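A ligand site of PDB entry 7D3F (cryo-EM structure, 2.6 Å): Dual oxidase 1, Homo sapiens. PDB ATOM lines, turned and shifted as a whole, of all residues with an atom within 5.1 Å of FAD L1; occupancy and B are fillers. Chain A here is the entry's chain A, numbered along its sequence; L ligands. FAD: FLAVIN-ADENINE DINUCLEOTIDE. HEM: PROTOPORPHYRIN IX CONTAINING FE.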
ATOM      1  N   ARG A1113     -16.856 -20.043  18.804  1.00  0.00           N
ATOM      2  CA  ARG A1113     -15.831 -19.990  17.771  1.00  0.00           C
ATOM      3  C   ARG A1113     -14.510 -20.575  18.269  1.00  0.00           C
ATOM      4  O   ARG A1113     -13.793 -21.225  17.499  1.00  0.00           O
ATOM      5  CB  ARG A1113     -15.631 -18.547  17.305  1.00  0.00           C
ATOM      6  CG  ARG A1113     -15.724 -18.366  15.798  1.00  0.00           C
ATOM      7  CD  ARG A1113     -15.422 -16.930  15.395  1.00  0.00           C
ATOM      8  NE  ARG A1113     -14.082 -16.521  15.800  1.00  0.00           N
ATOM      9  CZ  ARG A1113     -12.980 -16.794  15.106  1.00  0.00           C
ATOM     10  NH1 ARG A1113     -11.801 -16.378  15.546  1.00  0.00           N
ATOM     11  NH2 ARG A1113     -13.045 -17.483  13.981  1.00  0.00           N
ATOM     12  N   ASP A1124     -17.396 -19.686  11.281  1.00  0.00           N
ATOM     13  CA  ASP A1124     -17.084 -18.505  10.493  1.00  0.00           C
ATOM     14  C   ASP A1124     -17.859 -18.455   9.180  1.00  0.00           C
ATOM     15  O   ASP A1124     -17.992 -17.371   8.595  1.00  0.00           O
ATOM     16  CB  ASP A1124     -15.581 -18.426  10.192  1.00  0.00           C
ATOM     17  CG  ASP A1124     -14.764 -18.104  11.422  1.00  0.00           C
ATOM     18  OD1 ASP A1124     -13.768 -18.806  11.681  1.00  0.00           O
ATOM     19  OD2 ASP A1124     -15.122 -17.146  12.145  1.00  0.00           O
ATOM     20  N   ALA A1125     -18.379 -19.581   8.706  1.00  0.00           N
ATOM     21  CA  ALA A1125     -19.174 -19.632   7.493  1.00  0.00           C
ATOM     22  C   ALA A1125     -20.661 -19.440   7.762  1.00  0.00           C
ATOM     23  O   ALA A1125     -21.461 -19.533   6.820  1.00  0.00           O
ATOM     24  CB  ALA A1125     -18.947 -20.957   6.771  1.00  0.00           C
ATOM     25  N   VAL A1127     -22.761 -16.982   8.252  1.00  0.00           N
ATOM     26  CA  VAL A1127     -23.466 -16.045   7.376  1.00  0.00           C
ATOM     27  C   VAL A1127     -23.705 -16.672   6.006  1.00  0.00           C
ATOM     28  O   VAL A1127     -24.828 -16.682   5.491  1.00  0.00           O
ATOM     29  CB  VAL A1127     -22.690 -14.727   7.265  1.00  0.00           C
ATOM     30  CG1 VAL A1127     -23.306 -13.839   6.187  1.00  0.00           C
ATOM     31  CG2 VAL A1127     -22.666 -14.008   8.598  1.00  0.00           C
ATOM     32  N   ASP A1128     -22.643 -17.247   5.421  1.00  0.00           N
ATOM     33  CA  ASP A1128     -22.805 -17.966   4.163  1.00  0.00           C
ATOM     34  C   ASP A1128     -23.860 -19.060   4.297  1.00  0.00           C
ATOM     35  O   ASP A1128     -24.802 -19.140   3.494  1.00  0.00           O
ATOM     36  CB  ASP A1128     -21.474 -18.565   3.714  1.00  0.00           C
ATOM     37  CG  ASP A1128     -20.730 -17.675   2.746  1.00  0.00           C
ATOM     38  OD1 ASP A1128     -21.315 -16.665   2.290  1.00  0.00           O
ATOM     39  OD2 ASP A1128     -19.552 -17.970   2.441  1.00  0.00           O
ATOM     40  N   ARG A1131     -27.322 -17.675   3.984  1.00  0.00           N
ATOM     41  CA  ARG A1131     -27.785 -17.545   2.609  1.00  0.00           C
ATOM     42  C   ARG A1131     -28.189 -18.907   2.056  1.00  0.00           C
ATOM     43  O   ARG A1131     -29.279 -19.059   1.499  1.00  0.00           O
ATOM     44  CB  ARG A1131     -26.690 -16.922   1.743  1.00  0.00           C
ATOM     45  CG  ARG A1131     -26.388 -15.464   2.052  1.00  0.00           C
ATOM     46  CD  ARG A1131     -25.484 -14.859   0.991  1.00  0.00           C
ATOM     47  NE  ARG A1131     -25.187 -13.459   1.244  1.00  0.00           N
ATOM     48  CZ  ARG A1131     -24.108 -13.032   1.886  1.00  0.00           C
ATOM     49  NH1 ARG A1131     -23.211 -13.898   2.343  1.00  0.00           N
ATOM     50  NH2 ARG A1131     -23.913 -11.724   2.078  1.00  0.00           N
ATOM     51  N   HIS A1211     -27.279 -10.312  -4.100  1.00  0.00           N
ATOM     52  CA  HIS A1211     -25.963  -9.689  -4.218  1.00  0.00           C
ATOM     53  C   HIS A1211     -26.017  -8.418  -5.054  1.00  0.00           C
ATOM     54  O   HIS A1211     -25.419  -7.398  -4.703  1.00  0.00           O
ATOM     55  CB  HIS A1211     -24.970 -10.693  -4.807  1.00  0.00           C
ATOM     56  CG  HIS A1211     -23.599 -10.140  -5.037  1.00  0.00           C
ATOM     57  ND1 HIS A1211     -22.819  -9.639  -4.023  1.00  0.00           N
ATOM     58  CD2 HIS A1211     -22.863 -10.038  -6.165  1.00  0.00           C
ATOM     59  CE1 HIS A1211     -21.665  -9.241  -4.519  1.00  0.00           C
ATOM     60  NE2 HIS A1211     -21.665  -9.463  -5.819  1.00  0.00           N
ATOM     61  N   ARG A1214     -27.810  -5.689  -3.126  1.00  0.00           N
ATOM     62  CA  ARG A1214     -27.000  -5.344  -1.954  1.00  0.00           C
ATOM     63  C   ARG A1214     -25.837  -4.454  -2.362  1.00  0.00           C
ATOM     64  O   ARG A1214     -25.454  -3.539  -1.622  1.00  0.00           O
ATOM     65  CB  ARG A1214     -26.511  -6.610  -1.254  1.00  0.00           C
ATOM     66  CG  ARG A1214     -25.756  -6.352   0.041  1.00  0.00           C
ATOM     67  CD  ARG A1214     -25.617  -7.624   0.860  1.00  0.00           C
ATOM     68  NE  ARG A1214     -24.791  -7.426   2.045  1.00  0.00           N
ATOM     69  CZ  ARG A1214     -23.503  -7.741   2.118  1.00  0.00           C
ATOM     70  NH1 ARG A1214     -22.900  -8.289   1.075  1.00  0.00           N
ATOM     71  NH2 ARG A1214     -22.819  -7.527   3.235  1.00  0.00           N
ATOM     72  N   TRP A1305      -9.977  -9.790  17.672  1.00  0.00           N
ATOM     73  CA  TRP A1305     -10.656  -9.071  16.605  1.00  0.00           C
ATOM     74  C   TRP A1305     -11.781  -8.237  17.189  1.00  0.00           C
ATOM     75  O   TRP A1305     -12.349  -8.560  18.229  1.00  0.00           O
ATOM     76  CB  TRP A1305     -11.195 -10.037  15.540  1.00  0.00           C
ATOM     77  CG  TRP A1305     -12.070 -11.120  16.103  1.00  0.00           C
ATOM     78  CD1 TRP A1305     -11.664 -12.313  16.626  1.00  0.00           C
ATOM     79  CD2 TRP A1305     -13.498 -11.110  16.198  1.00  0.00           C
ATOM     80  NE1 TRP A1305     -12.750 -13.041  17.040  1.00  0.00           N
ATOM     81  CE2 TRP A1305     -13.882 -12.329  16.785  1.00  0.00           C
ATOM     82  CE3 TRP A1305     -14.489 -10.184  15.834  1.00  0.00           C
ATOM     83  CZ2 TRP A1305     -15.221 -12.647  17.027  1.00  0.00           C
ATOM     84  CZ3 TRP A1305     -15.812 -10.509  16.079  1.00  0.00           C
ATOM     85  CH2 TRP A1305     -16.166 -11.719  16.662  1.00  0.00           C
ATOM     86  N   TYR A1318     -22.360  -4.198  11.334  1.00  0.00           N
ATOM     87  CA  TYR A1318     -21.130  -4.500  12.055  1.00  0.00           C
ATOM     88  C   TYR A1318     -20.419  -5.664  11.391  1.00  0.00           C
ATOM     89  O   TYR A1318     -21.007  -6.729  11.184  1.00  0.00           O
ATOM     90  CB  TYR A1318     -21.419  -4.821  13.524  1.00  0.00           C
ATOM     91  CG  TYR A1318     -21.574  -3.604  14.387  1.00  0.00           C
ATOM     92  CD1 TYR A1318     -20.460  -2.883  14.797  1.00  0.00           C
ATOM     93  CD2 TYR A1318     -22.829  -3.162  14.793  1.00  0.00           C
ATOM     94  CE1 TYR A1318     -20.588  -1.755  15.594  1.00  0.00           C
ATOM     95  CE2 TYR A1318     -22.965  -2.039  15.589  1.00  0.00           C
ATOM     96  CZ  TYR A1318     -21.846  -1.342  15.979  1.00  0.00           C
ATOM     97  OH  TYR A1318     -21.979  -0.226  16.769  1.00  0.00           O
ATOM     98  N   HIS A1319     -19.139  -5.464  11.051  1.00  0.00           N
ATOM     99  CA  HIS A1319     -18.346  -6.500  10.429  1.00  0.00           C
ATOM    100  C   HIS A1319     -17.100  -6.790  11.259  1.00  0.00           C
ATOM    101  O   HIS A1319     -16.496  -5.854  11.805  1.00  0.00           O
ATOM    102  CB  HIS A1319     -17.941  -6.106   9.002  1.00  0.00           C
ATOM    103  CG  HIS A1319     -19.095  -6.004   8.060  1.00  0.00           C
ATOM    104  ND1 HIS A1319     -19.398  -6.979   7.140  1.00  0.00           N
ATOM    105  CD2 HIS A1319     -20.030  -5.033   7.895  1.00  0.00           C
ATOM    106  CE1 HIS A1319     -20.466  -6.620   6.445  1.00  0.00           C
ATOM    107  NE2 HIS A1319     -20.863  -5.449   6.886  1.00  0.00           N
ATOM    108  N   PRO A1320     -16.700  -8.052  11.377  1.00  0.00           N
ATOM    109  CA  PRO A1320     -15.540  -8.393  12.197  1.00  0.00           C
ATOM    110  C   PRO A1320     -14.235  -8.213  11.440  1.00  0.00           C
ATOM    111  O   PRO A1320     -14.125  -8.563  10.265  1.00  0.00           O
ATOM    112  CB  PRO A1320     -15.781  -9.864  12.552  1.00  0.00           C
ATOM    113  CG  PRO A1320     -16.527 -10.387  11.364  1.00  0.00           C
ATOM    114  CD  PRO A1320     -17.385  -9.247  10.855  1.00  0.00           C
ATOM    115  N   PHE A1321     -13.239  -7.681  12.139  1.00  0.00           N
ATOM    116  CA  PHE A1321     -11.912  -7.494  11.563  1.00  0.00           C
ATOM    117  C   PHE A1321     -10.867  -7.696  12.650  1.00  0.00           C
ATOM    118  O   PHE A1321     -11.033  -7.226  13.780  1.00  0.00           O
ATOM    119  CB  PHE A1321     -11.760  -6.114  10.921  1.00  0.00           C
ATOM    120  CG  PHE A1321     -12.667  -5.895   9.758  1.00  0.00           C
ATOM    121  CD1 PHE A1321     -12.424  -6.534   8.550  1.00  0.00           C
ATOM    122  CD2 PHE A1321     -13.770  -5.064   9.860  1.00  0.00           C
ATOM    123  CE1 PHE A1321     -13.255  -6.337   7.462  1.00  0.00           C
ATOM    124  CE2 PHE A1321     -14.601  -4.867   8.772  1.00  0.00           C
ATOM    125  CZ  PHE A1321     -14.352  -5.500   7.579  1.00  0.00           C
ATOM    126  N   THR A1322      -9.805  -8.412  12.298  1.00  0.00           N
ATOM    127  CA  THR A1322      -8.729  -8.693  13.234  1.00  0.00           C
ATOM    128  C   THR A1322      -7.860  -7.453  13.436  1.00  0.00           C
ATOM    129  O   THR A1322      -7.487  -6.783  12.469  1.00  0.00           O
ATOM    130  CB  THR A1322      -7.865  -9.848  12.731  1.00  0.00           C
ATOM    131  OG1 THR A1322      -8.688 -11.011  12.533  1.00  0.00           O
ATOM    132  CG2 THR A1322      -6.768 -10.177  13.729  1.00  0.00           C
ATOM    133  N   HIS A1335      -6.555  -4.028   8.570  1.00  0.00           N
ATOM    134  CA  HIS A1335      -6.272  -4.249   7.157  1.00  0.00           C
ATOM    135  C   HIS A1335      -7.454  -4.998   6.554  1.00  0.00           C
ATOM    136  O   HIS A1335      -7.575  -6.220   6.704  1.00  0.00           O
ATOM    137  CB  HIS A1335      -4.962  -5.017   6.966  1.00  0.00           C
ATOM    138  CG  HIS A1335      -3.736  -4.179   7.217  1.00  0.00           C
ATOM    139  ND1 HIS A1335      -3.193  -4.010   8.466  1.00  0.00           N
ATOM    140  CD2 HIS A1335      -2.967  -3.468   6.364  1.00  0.00           C
ATOM    141  CE1 HIS A1335      -2.125  -3.235   8.370  1.00  0.00           C
ATOM    142  NE2 HIS A1335      -1.971  -2.883   7.104  1.00  0.00           N
ATOM    143  N   ILE A1336      -8.318  -4.259   5.869  1.00  0.00           N
ATOM    144  CA  ILE A1336      -9.598  -4.773   5.389  1.00  0.00           C
ATOM    145  C   ILE A1336      -9.472  -5.048   3.886  1.00  0.00           C
ATOM    146  O   ILE A1336      -9.124  -4.159   3.110  1.00  0.00           O
ATOM    147  CB  ILE A1336     -10.729  -3.774   5.669  1.00  0.00           C
ATOM    148  CG1 ILE A1336     -10.911  -3.622   7.189  1.00  0.00           C
ATOM    149  CG2 ILE A1336     -12.015  -4.220   4.994  1.00  0.00           C
ATOM    150  CD1 ILE A1336     -11.730  -2.425   7.590  1.00  0.00           C
ATOM    151  N   ARG A1337      -9.746  -6.284   3.489  1.00  0.00           N
ATOM    152  CA  ARG A1337      -9.693  -6.673   2.093  1.00  0.00           C
ATOM    153  C   ARG A1337     -11.023  -6.386   1.410  1.00  0.00           C
ATOM    154  O   ARG A1337     -12.089  -6.488   2.024  1.00  0.00           O
ATOM    155  CB  ARG A1337      -9.343  -8.155   1.968  1.00  0.00           C
ATOM    156  CG  ARG A1337      -8.071  -8.564   2.683  1.00  0.00           C
ATOM    157  CD  ARG A1337      -7.820 -10.056   2.545  1.00  0.00           C
ATOM    158  NE  ARG A1337      -8.946 -10.844   3.019  1.00  0.00           N
ATOM    159  CZ  ARG A1337      -9.094 -11.260   4.272  1.00  0.00           C
ATOM    160  NH1 ARG A1337      -8.180 -10.962   5.188  1.00  0.00           N
ATOM    161  NH2 ARG A1337     -10.154 -11.980   4.618  1.00  0.00           N
ATOM    162  N   ALA A1339     -13.637  -7.620  -0.136  1.00  0.00           N
ATOM    163  CA  ALA A1339     -14.269  -8.924  -0.327  1.00  0.00           C
ATOM    164  C   ALA A1339     -15.639  -8.831  -0.976  1.00  0.00           C
ATOM    165  O   ALA A1339     -16.013  -9.741  -1.729  1.00  0.00           O
ATOM    166  CB  ALA A1339     -14.394  -9.648   1.022  1.00  0.00           C
ATOM    167  N   GLY A1340     -16.402  -7.779  -0.707  1.00  0.00           N
ATOM    168  CA  GLY A1340     -17.723  -7.648  -1.265  1.00  0.00           C
ATOM    169  C   GLY A1340     -18.264  -6.228  -1.198  1.00  0.00           C
ATOM    170  O   GLY A1340     -17.513  -5.249  -1.247  1.00  0.00           O
ATOM    171  N   PRO A1341     -19.588  -6.098  -1.100  1.00  0.00           N
ATOM    172  CA  PRO A1341     -20.196  -4.761  -1.125  1.00  0.00           C
ATOM    173  C   PRO A1341     -19.740  -3.846   0.009  1.00  0.00           C
ATOM    174  O   PRO A1341     -19.298  -2.725  -0.254  1.00  0.00           O
ATOM    175  CB  PRO A1341     -21.702  -5.064  -1.047  1.00  0.00           C
ATOM    176  CG  PRO A1341     -21.832  -6.457  -1.564  1.00  0.00           C
ATOM    177  CD  PRO A1341     -20.602  -7.174  -1.111  1.00  0.00           C
ATOM    178  N   TRP A1342     -19.840  -4.301   1.255  1.00  0.00           N
ATOM    179  CA  TRP A1342     -19.529  -3.416   2.379  1.00  0.00           C
ATOM    180  C   TRP A1342     -18.076  -2.981   2.369  1.00  0.00           C
ATOM    181  O   TRP A1342     -17.767  -1.808   2.587  1.00  0.00           O
ATOM    182  CB  TRP A1342     -19.876  -4.099   3.706  1.00  0.00           C
ATOM    183  CG  TRP A1342     -19.889  -3.172   4.872  1.00  0.00           C
ATOM    184  CD1 TRP A1342     -20.941  -2.432   5.318  1.00  0.00           C
ATOM    185  CD2 TRP A1342     -18.790  -2.883   5.755  1.00  0.00           C
ATOM    186  NE1 TRP A1342     -20.573  -1.696   6.424  1.00  0.00           N
ATOM    187  CE2 TRP A1342     -19.246  -1.960   6.708  1.00  0.00           C
ATOM    188  CE3 TRP A1342     -17.460  -3.323   5.822  1.00  0.00           C
ATOM    189  CZ2 TRP A1342     -18.434  -1.455   7.727  1.00  0.00           C
ATOM    190  CZ3 TRP A1342     -16.654  -2.825   6.826  1.00  0.00           C
ATOM    191  CH2 TRP A1342     -17.142  -1.905   7.761  1.00  0.00           C
ATOM    192  N   THR A1343     -17.159  -3.922   2.117  1.00  0.00           N
ATOM    193  CA  THR A1343     -15.735  -3.572   2.092  1.00  0.00           C
ATOM    194  C   THR A1343     -15.405  -2.642   0.934  1.00  0.00           C
ATOM    195  O   THR A1343     -14.611  -1.697   1.106  1.00  0.00           O
ATOM    196  CB  THR A1343     -14.890  -4.853   2.010  1.00  0.00           C
ATOM    197  OG1 THR A1343     -15.370  -5.684   0.949  1.00  0.00           O
ATOM    198  CG2 THR A1343     -14.959  -5.622   3.318  1.00  0.00           C
ATOM    199  N   THR A1344     -15.984  -2.882  -0.239  1.00  0.00           N
ATOM    200  CA  THR A1344     -15.734  -1.997  -1.377  1.00  0.00           C
ATOM    201  C   THR A1344     -16.265  -0.592  -1.102  1.00  0.00           C
ATOM    202  O   THR A1344     -15.599   0.401  -1.411  1.00  0.00           O
ATOM    203  CB  THR A1344     -16.371  -2.570  -2.643  1.00  0.00           C
ATOM    204  OG1 THR A1344     -15.823  -3.872  -2.897  1.00  0.00           O
ATOM    205  CG2 THR A1344     -16.084  -1.677  -3.840  1.00  0.00           C
ATOM    206  N   THR A1393      -3.487 -12.884   9.124  1.00  0.00           N
ATOM    207  CA  THR A1393      -3.650 -11.498   9.568  1.00  0.00           C
ATOM    208  C   THR A1393      -3.327 -11.298  11.038  1.00  0.00           C
ATOM    209  O   THR A1393      -2.597 -10.335  11.365  1.00  0.00           O
ATOM    210  CB  THR A1393      -5.063 -11.026   9.240  1.00  0.00           C
ATOM    211  OG1 THR A1393      -5.345 -11.252   7.855  1.00  0.00           O
ATOM    212  CG2 THR A1393      -5.221  -9.545   9.547  1.00  0.00           C
ATOM    213  N   PHE A1551      -7.759 -17.416  15.619  1.00  0.00           N
ATOM    214  CA  PHE A1551      -7.881 -15.979  15.839  1.00  0.00           C
ATOM    215  C   PHE A1551      -8.769 -15.326  14.782  1.00  0.00           C
ATOM    216  O   PHE A1551      -8.957 -15.855  13.680  1.00  0.00           O
ATOM    217  CB  PHE A1551      -6.517 -15.300  15.826  1.00  0.00           C
ATOM    218  CG  PHE A1551      -5.425 -16.085  16.513  1.00  0.00           C
ATOM    219  CD1 PHE A1551      -5.357 -16.162  17.886  1.00  0.00           C
ATOM    220  CD2 PHE A1551      -4.446 -16.725  15.763  1.00  0.00           C
ATOM    221  CE1 PHE A1551      -4.361 -16.876  18.516  1.00  0.00           C
ATOM    222  CE2 PHE A1551      -3.439 -17.435  16.380  1.00  0.00           C
ATOM    223  CZ  PHE A1551      -3.395 -17.510  17.750  1.00  0.00           C
ATOM    224  OXT PHE A1551      -9.329 -14.250  14.998  1.00  0.00           O
HETATM  225  PA  FAD L   1     -19.809  -9.923   1.433  1.00  0.00           P
HETATM  226  O1A FAD L   1     -20.790  -9.971   2.571  1.00  0.00           O
HETATM  227  O2A FAD L   1     -20.301 -10.087   0.012  1.00  0.00           O
HETATM  228  O5B FAD L   1     -18.706 -11.068   1.667  1.00  0.00           O
HETATM  229  C5B FAD L   1     -19.054 -12.440   1.506  1.00  0.00           C
HETATM  230  C4B FAD L   1     -18.244 -13.279   2.486  1.00  0.00           C
HETATM  231  O4B FAD L   1     -17.959 -12.496   3.659  1.00  0.00           O
HETATM  232  C3B FAD L   1     -19.026 -14.494   2.929  1.00  0.00           C
HETATM  233  O3B FAD L   1     -18.239 -15.679   2.745  1.00  0.00           O
HETATM  234  C2B FAD L   1     -19.317 -14.288   4.399  1.00  0.00           C
HETATM  235  O2B FAD L   1     -19.039 -15.485   5.134  1.00  0.00           O
HETATM  236  C1B FAD L   1     -18.389 -13.170   4.840  1.00  0.00           C
HETATM  237  N9A FAD L   1     -19.125 -12.215   5.706  1.00  0.00           N
HETATM  238  C8A FAD L   1     -19.866 -11.164   5.271  1.00  0.00           C
HETATM  239  N7A FAD L   1     -20.406 -10.489   6.312  1.00  0.00           N
HETATM  240  C5A FAD L   1     -20.015 -11.092   7.440  1.00  0.00           C
HETATM  241  C6A FAD L   1     -20.222 -10.887   8.891  1.00  0.00           C
HETATM  242  N6A FAD L   1     -20.982  -9.856   9.353  1.00  0.00           N
HETATM  243  N1A FAD L   1     -19.628 -11.753   9.745  1.00  0.00           N
HETATM  244  C2A FAD L   1     -18.870 -12.766   9.310  1.00  0.00           C
HETATM  245  N3A FAD L   1     -18.631 -13.012   7.999  1.00  0.00           N
HETATM  246  C4A FAD L   1     -19.167 -12.221   7.041  1.00  0.00           C
HETATM  247  N1  FAD L   1     -11.471  -9.480   6.791  1.00  0.00           N
HETATM  248  C2  FAD L   1     -10.446  -8.604   6.644  1.00  0.00           C
HETATM  249  O2  FAD L   1     -10.283  -8.066   5.532  1.00  0.00           O
HETATM  250  N3  FAD L   1      -9.609  -8.293   7.649  1.00  0.00           N
HETATM  251  C4  FAD L   1      -9.712  -8.835   8.869  1.00  0.00           C
HETATM  252  O4  FAD L   1      -8.916  -8.534   9.776  1.00  0.00           O
HETATM  253  C4X FAD L   1     -10.805  -9.809   9.109  1.00  0.00           C
HETATM  254  N5  FAD L   1     -10.988 -10.391  10.312  1.00  0.00           N
HETATM  255  C5X FAD L   1     -11.991 -11.274  10.512  1.00  0.00           C
HETATM  256  C6  FAD L   1     -12.139 -11.863  11.763  1.00  0.00           C
HETATM  257  C7  FAD L   1     -13.159 -12.762  11.996  1.00  0.00           C
HETATM  258  C7M FAD L   1     -13.317 -13.395  13.361  1.00  0.00           C
HETATM  259  C8  FAD L   1     -14.100 -13.118  10.900  1.00  0.00           C
HETATM  260  C8M FAD L   1     -15.210 -14.102  11.139  1.00  0.00           C
HETATM  261  C9  FAD L   1     -13.945 -12.541   9.651  1.00  0.00           C
HETATM  262  C9A FAD L   1     -12.936 -11.618   9.401  1.00  0.00           C
HETATM  263  N10 FAD L   1     -12.772 -11.013   8.131  1.00  0.00           N
HETATM  264  C10 FAD L   1     -11.706 -10.105   7.967  1.00  0.00           C
HETATM  265  C1' FAD L   1     -13.643 -11.300   6.985  1.00  0.00           C
HETATM  266  C2' FAD L   1     -15.069 -10.768   7.167  1.00  0.00           C
HETATM  267  O2' FAD L   1     -15.985 -11.737   6.653  1.00  0.00           O
HETATM  268  C3' FAD L   1     -15.312  -9.428   6.490  1.00  0.00           C
HETATM  269  O3' FAD L   1     -16.053  -8.583   7.365  1.00  0.00           O
HETATM  270  C4' FAD L   1     -16.092  -9.643   5.197  1.00  0.00           C
HETATM  271  O4' FAD L   1     -15.183  -9.976   4.145  1.00  0.00           O
HETATM  272  C5' FAD L   1     -16.899  -8.413   4.792  1.00  0.00           C
HETATM  273  O5' FAD L   1     -17.650  -8.779   3.636  1.00  0.00           O
HETATM  274  P   FAD L   1     -18.668  -7.775   2.881  1.00  0.00           P
HETATM  275  O1P FAD L   1     -19.954  -7.702   3.670  1.00  0.00           O
HETATM  276  O2P FAD L   1     -17.947  -6.497   2.536  1.00  0.00           O
HETATM  277  O3P FAD L   1     -18.897  -8.595   1.517  1.00  0.00           O
HETATM  278  CHA HEM L   2     -29.212 -10.976   8.433  1.00  0.00           C
HETATM  279  CHB HEM L   2     -33.254 -13.669   8.538  1.00  0.00           C
HETATM  280  CHC HEM L   2     -32.844 -14.403   3.759  1.00  0.00           C
HETATM  281  CHD HEM L   2     -28.439 -12.382   3.846  1.00  0.00           C
HETATM  282  C1A HEM L   2     -30.365 -11.600   8.885  1.00  0.00           C
HETATM  283  C2A HEM L   2     -30.915 -11.545  10.226  1.00  0.00           C
HETATM  284  C3A HEM L   2     -32.025 -12.277  10.251  1.00  0.00           C
HETATM  285  C4A HEM L   2     -32.224 -12.844   8.927  1.00  0.00           C
HETATM  286  CMA HEM L   2     -32.947 -12.496  11.472  1.00  0.00           C
HETATM  287  CAA HEM L   2     -30.331 -10.754  11.415  1.00  0.00           C
HETATM  288  CBA HEM L   2     -30.591  -9.267  11.238  1.00  0.00           C
HETATM  289  CGA HEM L   2     -30.044  -8.508  12.416  1.00  0.00           C
HETATM  290  O1A HEM L   2     -29.469  -9.163  13.333  1.00  0.00           O
HETATM  291  O2A HEM L   2     -30.189  -7.269  12.453  1.00  0.00           O
HETATM  292  C1B HEM L   2     -33.544 -14.032   7.233  1.00  0.00           C
HETATM  293  C2B HEM L   2     -34.781 -14.617   6.761  1.00  0.00           C
HETATM  294  C3B HEM L   2     -34.657 -14.826   5.441  1.00  0.00           C
HETATM  295  C4B HEM L   2     -33.344 -14.358   5.034  1.00  0.00           C
HETATM  296  CMB HEM L   2     -35.988 -14.930   7.683  1.00  0.00           C
HETATM  297  CAB HEM L   2     -35.665 -15.414   4.414  1.00  0.00           C
HETATM  298  CBB HEM L   2     -36.962 -15.568   4.651  1.00  0.00           C
HETATM  299  C1C HEM L   2     -31.608 -13.923   3.350  1.00  0.00           C
HETATM  300  C2C HEM L   2     -31.093 -13.935   1.990  1.00  0.00           C
HETATM  301  C3C HEM L   2     -29.867 -13.367   2.019  1.00  0.00           C
HETATM  302  C4C HEM L   2     -29.592 -12.991   3.392  1.00  0.00           C
HETATM  303  CMC HEM L   2     -31.877 -14.514   0.798  1.00  0.00           C
HETATM  304  CAC HEM L   2     -28.857 -13.130   0.859  1.00  0.00           C
HETATM  305  CBC HEM L   2     -29.041 -13.500  -0.411  1.00  0.00           C
HETATM  306  C1D HEM L   2     -28.290 -11.773   5.077  1.00  0.00           C
HETATM  307  C2D HEM L   2     -27.195 -10.900   5.467  1.00  0.00           C
HETATM  308  C3D HEM L   2     -27.397 -10.512   6.729  1.00  0.00           C
HETATM  309  C4D HEM L   2     -28.633 -11.119   7.199  1.00  0.00           C
HETATM  310  CMD HEM L   2     -25.997 -10.499   4.576  1.00  0.00           C
HETATM  311  CAD HEM L   2     -26.468  -9.580   7.538  1.00  0.00           C
HETATM  312  CBD HEM L   2     -25.862 -10.332   8.711  1.00  0.00           C
HETATM  313  CGD HEM L   2     -24.955  -9.416   9.490  1.00  0.00           C
HETATM  314  O1D HEM L   2     -24.754  -8.250   9.045  1.00  0.00           O
HETATM  315  O2D HEM L   2     -24.430  -9.839  10.551  1.00  0.00           O
HETATM  316  NA  HEM L   2     -31.188 -12.407   8.122  1.00  0.00           N
HETATM  317  NB  HEM L   2     -32.697 -13.891   6.161  1.00  0.00           N
HETATM  318  NC  HEM L   2     -30.672 -13.332   4.168  1.00  0.00           N
HETATM  319  ND  HEM L   2     -29.147 -11.877   6.153  1.00  0.00           N
HETATM  320 FE   HEM L   2     -30.929 -12.872   6.149  1.00  0.00          FE
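O1A of FAD L1 lies within salt-bridge range of NH2 of Arg 1131 (3.6 Å).
An oxygen (O2P) of FAD L1 is in hydrogen-bond range of the side-chain hydroxyl of Thr 1343, at 3.1 Å.
An oxygen (O2P) of FAD L1 sits at hydrogen-bond distance from the backbone NH (N) of Trp 1342, at 3.2 Å.
OG1 of Thr 1322 sits at hydrogen-bond distance from N5 of FAD L1, 3.3 Å away.
N3 of FAD L1 lies within hydrogen-bond range of O of His 1335 (3.1 Å).
The backbone carbonyl oxygen of Pro 1320 lies close to an oxygen (O3') of FAD L1 (3.5 Å).
An oxygen (O2) of FAD L1 lies within hydrogen-bond range of the backbone NH of Arg 1337, at 2.8 Å.
The backbone NH (N) of Gly 1340 lies close to an oxygen (O3P) of FAD L1.
O3B of FAD L1 sits at hydrogen-bond distance from OD2 of Asp 1128.
The backbone NH (N) of Thr 1322 sits at hydrogen-bond distance from an oxygen (O4) of FAD L1 (2.7 Å).
The guanidinium group of Arg 1214 is in salt-bridge range of an oxygen (O1P) of FAD L1 (2.9 Å).
The backbone NH (N) of Thr 1343 is in hydrogen-bond range of an oxygen (O2P) of FAD L1 (2.7 Å).
The backbone carbonyl oxygen (O) of Gly 1340 lies within hydrogen-bond range of the side-chain hydroxyl (OG1) of Thr 1344, at 2.7 Å.
The guanidinium group of Arg 1113 is in salt-bridge range of the chain-end carboxylate of Phe 1551, 3.3 Å away.
The backbone NH (N) of Gly 1340 is in hydrogen-bond range of the side-chain hydroxyl (OG1) of Thr 1343.
The side-chain carboxylate (OD1) of Asp 1124 is in salt-bridge range of the guanidinium group (NH2) of Arg 1113 (2.8 Å).
The side-chain hydroxyl of Thr 1343 sits at hydrogen-bond distance from the backbone NH of Ala 1339 (2.8 Å).
The side-chain carboxylate of Asp 1128 is in salt-bridge range of the guanidinium group of Arg 1131 (3.4 Å).
Arg 1113 touches FAD L1 (CZ to C7M, 3.8 Å).
OD2 of Asp 1124 touches C8M of FAD L1, 3.2 Å away.
CG2 of Val 1127 touches N1A of FAD L1 (3.95 Å).
Trp 1305 touches FAD L1.
O of Tyr 1318 touches N6A of FAD L1, 3.6 Å away.
CE1 of His 1319 touches O1P of FAD L1 (3.0 Å).
CA of Phe 1321 touches N5 of FAD L1, at 3.3 Å.
Ile 1336 touches FAD L1.
CB of Ala 1339 touches O4' of FAD L1, 3.2 Å away.
CD of Pro 1341 touches O2A of FAD L1, 3.1 Å away.
CG2 of Thr 1393 touches O4 of FAD L1, 3.8 Å away.
Hydrophobic or aromatic side chains within 4 Å of FAD L1: Val 1127, Trp 1305, His 1319, Pro 1320, Phe 1321, Ala 1339, Pro 1341 and Trp 1342.
Within 4 Å of FAD L1: Arg 1113, Asp 1124, Val 1127, Asp 1128, Arg 1131, Arg 1214, Trp 1305, Tyr 1318, His 1319, Pro 1320, Phe 1321, Thr 1322, His 1335, Ile 1336, Arg 1337, Ala 1339, Gly 1340, Pro 1341, Trp 1342, Thr 1343 and Thr 1393.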
